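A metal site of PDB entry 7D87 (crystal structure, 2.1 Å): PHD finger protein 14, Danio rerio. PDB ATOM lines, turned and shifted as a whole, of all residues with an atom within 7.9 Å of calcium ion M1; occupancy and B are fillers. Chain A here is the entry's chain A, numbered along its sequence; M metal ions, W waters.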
ATOM      1  N   LEU A  77      30.975  18.839  22.978  1.00  0.00           N
ATOM      2  CA  LEU A  77      31.274  17.572  22.315  1.00  0.00           C
ATOM      3  C   LEU A  77      31.969  17.717  20.957  1.00  0.00           C
ATOM      4  O   LEU A  77      32.240  16.686  20.321  1.00  0.00           O
ATOM      5  CB  LEU A  77      29.976  16.755  22.155  1.00  0.00           C
ATOM      6  CG  LEU A  77      29.233  16.355  23.432  1.00  0.00           C
ATOM      7  CD1 LEU A  77      27.878  15.746  23.097  1.00  0.00           C
ATOM      8  CD2 LEU A  77      30.049  15.374  24.225  1.00  0.00           C
ATOM      9  N   VAL A  96      22.325  19.913  19.423  1.00  0.00           N
ATOM     10  CA  VAL A  96      21.303  18.862  19.363  1.00  0.00           C
ATOM     11  C   VAL A  96      21.855  17.645  18.627  1.00  0.00           C
ATOM     12  O   VAL A  96      21.696  16.497  19.055  1.00  0.00           O
ATOM     13  CB  VAL A  96      20.029  19.395  18.684  1.00  0.00           C
ATOM     14  CG1 VAL A  96      19.030  18.251  18.476  1.00  0.00           C
ATOM     15  CG2 VAL A  96      19.409  20.492  19.517  1.00  0.00           C
ATOM     16  N   VAL A  97      22.519  17.892  17.496  1.00  0.00           N
ATOM     17  CA  VAL A  97      22.956  16.768  16.661  1.00  0.00           C
ATOM     18  C   VAL A  97      24.007  15.938  17.408  1.00  0.00           C
ATOM     19  O   VAL A  97      23.954  14.699  17.393  1.00  0.00           O
ATOM     20  CB  VAL A  97      23.447  17.284  15.287  1.00  0.00           C
ATOM     21  CG1 VAL A  97      24.857  17.905  15.345  1.00  0.00           C
ATOM     22  CG2 VAL A  97      23.363  16.213  14.237  1.00  0.00           C
ATOM     23  N   CYS A  98      24.925  16.587  18.135  1.00  0.00           N
ATOM     24  CA  CYS A  98      25.904  15.827  18.907  1.00  0.00           C
ATOM     25  C   CYS A  98      25.244  15.014  20.012  1.00  0.00           C
ATOM     26  O   CYS A  98      25.588  13.846  20.233  1.00  0.00           O
ATOM     27  CB  CYS A  98      26.962  16.750  19.521  1.00  0.00           C
ATOM     28  SG  CYS A  98      28.126  17.440  18.310  1.00  0.00           S
ATOM     29  N   ALA A  99      24.259  15.604  20.684  1.00  0.00           N
ATOM     30  CA  ALA A  99      23.535  14.883  21.724  1.00  0.00           C
ATOM     31  C   ALA A  99      22.819  13.674  21.164  1.00  0.00           C
ATOM     32  O   ALA A  99      22.786  12.612  21.791  1.00  0.00           O
ATOM     33  CB  ALA A  99      22.552  15.828  22.424  1.00  0.00           C
ATOM     34  N   LEU A 100      22.250  13.794  19.953  1.00  0.00           N
ATOM     35  CA  LEU A 100      21.552  12.655  19.354  1.00  0.00           C
ATOM     36  C   LEU A 100      22.521  11.514  19.026  1.00  0.00           C
ATOM     37  O   LEU A 100      22.221  10.340  19.305  1.00  0.00           O
ATOM     38  CB  LEU A 100      20.812  13.094  18.080  1.00  0.00           C
ATOM     39  CG  LEU A 100      19.597  14.000  18.294  1.00  0.00           C
ATOM     40  CD1 LEU A 100      19.063  14.525  16.972  1.00  0.00           C
ATOM     41  CD2 LEU A 100      18.489  13.285  19.088  1.00  0.00           C
ATOM     42  N   TYR A 101      23.686  11.818  18.449  1.00  0.00           N
ATOM     43  CA  TYR A 101      24.534  10.774  17.911  1.00  0.00           C
ATOM     44  C   TYR A 101      25.570  10.224  18.906  1.00  0.00           C
ATOM     45  O   TYR A 101      26.012   9.092  18.732  1.00  0.00           O
ATOM     46  CB  TYR A 101      25.244  11.290  16.631  1.00  0.00           C
ATOM     47  CG  TYR A 101      24.310  11.272  15.417  1.00  0.00           C
ATOM     48  CD1 TYR A 101      23.437  12.313  15.162  1.00  0.00           C
ATOM     49  CD2 TYR A 101      24.259  10.166  14.570  1.00  0.00           C
ATOM     50  CE1 TYR A 101      22.559  12.267  14.072  1.00  0.00           C
ATOM     51  CE2 TYR A 101      23.402  10.118  13.492  1.00  0.00           C
ATOM     52  CZ  TYR A 101      22.544  11.176  13.247  1.00  0.00           C
ATOM     53  OH  TYR A 101      21.682  11.114  12.168  1.00  0.00           O
ATOM     54  N   VAL A 102      25.951  10.969  19.937  1.00  0.00           N
ATOM     55  CA  VAL A 102      26.993  10.472  20.852  1.00  0.00           C
ATOM     56  C   VAL A 102      26.364   9.485  21.820  1.00  0.00           C
ATOM     57  O   VAL A 102      25.362   9.812  22.483  1.00  0.00           O
ATOM     58  CB  VAL A 102      27.655  11.624  21.589  1.00  0.00           C
ATOM     59  CG1 VAL A 102      28.459  11.089  22.768  1.00  0.00           C
ATOM     60  CG2 VAL A 102      28.581  12.392  20.632  1.00  0.00           C
ATOM     61  N   PRO A 103      26.918   8.287  21.955  1.00  0.00           N
ATOM     62  CA  PRO A 103      26.360   7.315  22.897  1.00  0.00           C
ATOM     63  C   PRO A 103      26.457   7.804  24.343  1.00  0.00           C
ATOM     64  O   PRO A 103      27.347   8.559  24.717  1.00  0.00           O
ATOM     65  CB  PRO A 103      27.215   6.059  22.682  1.00  0.00           C
ATOM     66  CG  PRO A 103      28.456   6.548  21.989  1.00  0.00           C
ATOM     67  CD  PRO A 103      28.076   7.760  21.213  1.00  0.00           C
ATOM     68  N   GLY A 104      25.490   7.400  25.134  1.00  0.00           N
ATOM     69  CA  GLY A 104      25.483   7.806  26.524  1.00  0.00           C
ATOM     70  C   GLY A 104      24.977   9.206  26.791  1.00  0.00           C
ATOM     71  O   GLY A 104      24.998   9.636  27.942  1.00  0.00           O
ATOM     72  N   VAL A 105      24.519   9.930  25.774  1.00  0.00           N
ATOM     73  CA  VAL A 105      23.938  11.257  25.966  1.00  0.00           C
ATOM     74  C   VAL A 105      22.464  11.159  25.629  1.00  0.00           C
ATOM     75  O   VAL A 105      22.101  10.593  24.597  1.00  0.00           O
ATOM     76  CB  VAL A 105      24.626  12.324  25.112  1.00  0.00           C
ATOM     77  CG1 VAL A 105      24.066  13.716  25.426  1.00  0.00           C
ATOM     78  CG2 VAL A 105      26.133  12.270  25.332  1.00  0.00           C
ATOM     79  N   ALA A 106      21.615  11.669  26.501  1.00  0.00           N
ATOM     80  CA  ALA A 106      20.184  11.508  26.368  1.00  0.00           C
ATOM     81  C   ALA A 106      19.511  12.826  26.715  1.00  0.00           C
ATOM     82  O   ALA A 106      20.070  13.660  27.437  1.00  0.00           O
ATOM     83  CB  ALA A 106      19.655  10.407  27.283  1.00  0.00           C
ATOM     84  N   PHE A 107      18.296  13.003  26.213  1.00  0.00           N
ATOM     85  CA  PHE A 107      17.514  14.193  26.513  1.00  0.00           C
ATOM     86  C   PHE A 107      16.657  13.984  27.761  1.00  0.00           C
ATOM     87  O   PHE A 107      16.138  12.886  28.005  1.00  0.00           O
ATOM     88  CB  PHE A 107      16.645  14.564  25.321  1.00  0.00           C
ATOM     89  CG  PHE A 107      17.421  15.163  24.185  1.00  0.00           C
ATOM     90  CD1 PHE A 107      17.721  16.517  24.175  1.00  0.00           C
ATOM     91  CD2 PHE A 107      17.870  14.380  23.148  1.00  0.00           C
ATOM     92  CE1 PHE A 107      18.429  17.083  23.145  1.00  0.00           C
ATOM     93  CE2 PHE A 107      18.578  14.946  22.108  1.00  0.00           C
ATOM     94  CZ  PHE A 107      18.868  16.296  22.117  1.00  0.00           C
ATOM     95  N   ASN A 122      30.696  10.623  29.854  1.00  0.00           N
ATOM     96  CA  ASN A 122      30.835  11.417  28.635  1.00  0.00           C
ATOM     97  C   ASN A 122      32.142  12.179  28.645  1.00  0.00           C
ATOM     98  O   ASN A 122      32.866  12.217  27.641  1.00  0.00           O
ATOM     99  CB  ASN A 122      29.667  12.403  28.470  1.00  0.00           C
ATOM    100  CG  ASN A 122      28.318  11.722  28.477  1.00  0.00           C
ATOM    101  OD1 ASN A 122      27.397  12.175  29.134  1.00  0.00           O
ATOM    102  ND2 ASN A 122      28.210  10.631  27.756  1.00  0.00           N
ATOM    103  N   ASP A 179      18.243   2.419  18.679  1.00  0.00           N
ATOM    104  CA  ASP A 179      19.004   3.640  18.450  1.00  0.00           C
ATOM    105  C   ASP A 179      18.974   3.966  16.962  1.00  0.00           C
ATOM    106  O   ASP A 179      19.776   3.421  16.197  1.00  0.00           O
ATOM    107  CB  ASP A 179      20.449   3.507  18.927  1.00  0.00           C
ATOM    108  CG  ASP A 179      21.284   4.721  18.593  1.00  0.00           C
ATOM    109  OD1 ASP A 179      20.688   5.802  18.305  1.00  0.00           O
ATOM    110  OD2 ASP A 179      22.541   4.598  18.616  1.00  0.00           O
ATOM    111  N   PHE A 181      19.876   6.616  15.239  1.00  0.00           N
ATOM    112  CA  PHE A 181      20.882   7.502  14.677  1.00  0.00           C
ATOM    113  C   PHE A 181      22.170   6.710  14.487  1.00  0.00           C
ATOM    114  O   PHE A 181      22.655   6.068  15.426  1.00  0.00           O
ATOM    115  CB  PHE A 181      21.089   8.722  15.584  1.00  0.00           C
ATOM    116  CG  PHE A 181      19.798   9.442  15.905  1.00  0.00           C
ATOM    117  CD1 PHE A 181      19.235  10.313  14.999  1.00  0.00           C
ATOM    118  CD2 PHE A 181      19.139   9.200  17.116  1.00  0.00           C
ATOM    119  CE1 PHE A 181      18.024  10.944  15.276  1.00  0.00           C
ATOM    120  CE2 PHE A 181      17.936   9.835  17.412  1.00  0.00           C
ATOM    121  CZ  PHE A 181      17.375  10.705  16.477  1.00  0.00           C
HETATM  122 CA    CA M   1      22.677  10.170  22.283  1.00  0.00          CA
HETATM  123 CA    CA M   2      24.151   6.106  17.298  1.00  0.00          CA
HETATM  124  O   HOH W   1      19.846  10.061  21.596  1.00  0.00           O
HETATM  125  O   HOH W   2      22.585   7.796  22.074  1.00  0.00           O
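Of the 16 residues printed, 4 come within 4 Å of calcium ion M1.
Water W2 binds calcium ion M1 (2.4 Å).
O of Val 105 binds calcium ion M1, 2.4 Å away.
Calcium ion M1 is bound by O of Ala 99, at 2.5 Å.
O of Val 102 binds calcium ion M1.
Calcium ion M1 has four donor atoms within binding distance.
Slightly farther from calcium ion M1 lies water W1 (2.9 Å).
Slightly farther from calcium ion M1 lies O of Leu 100 (3.0 Å).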
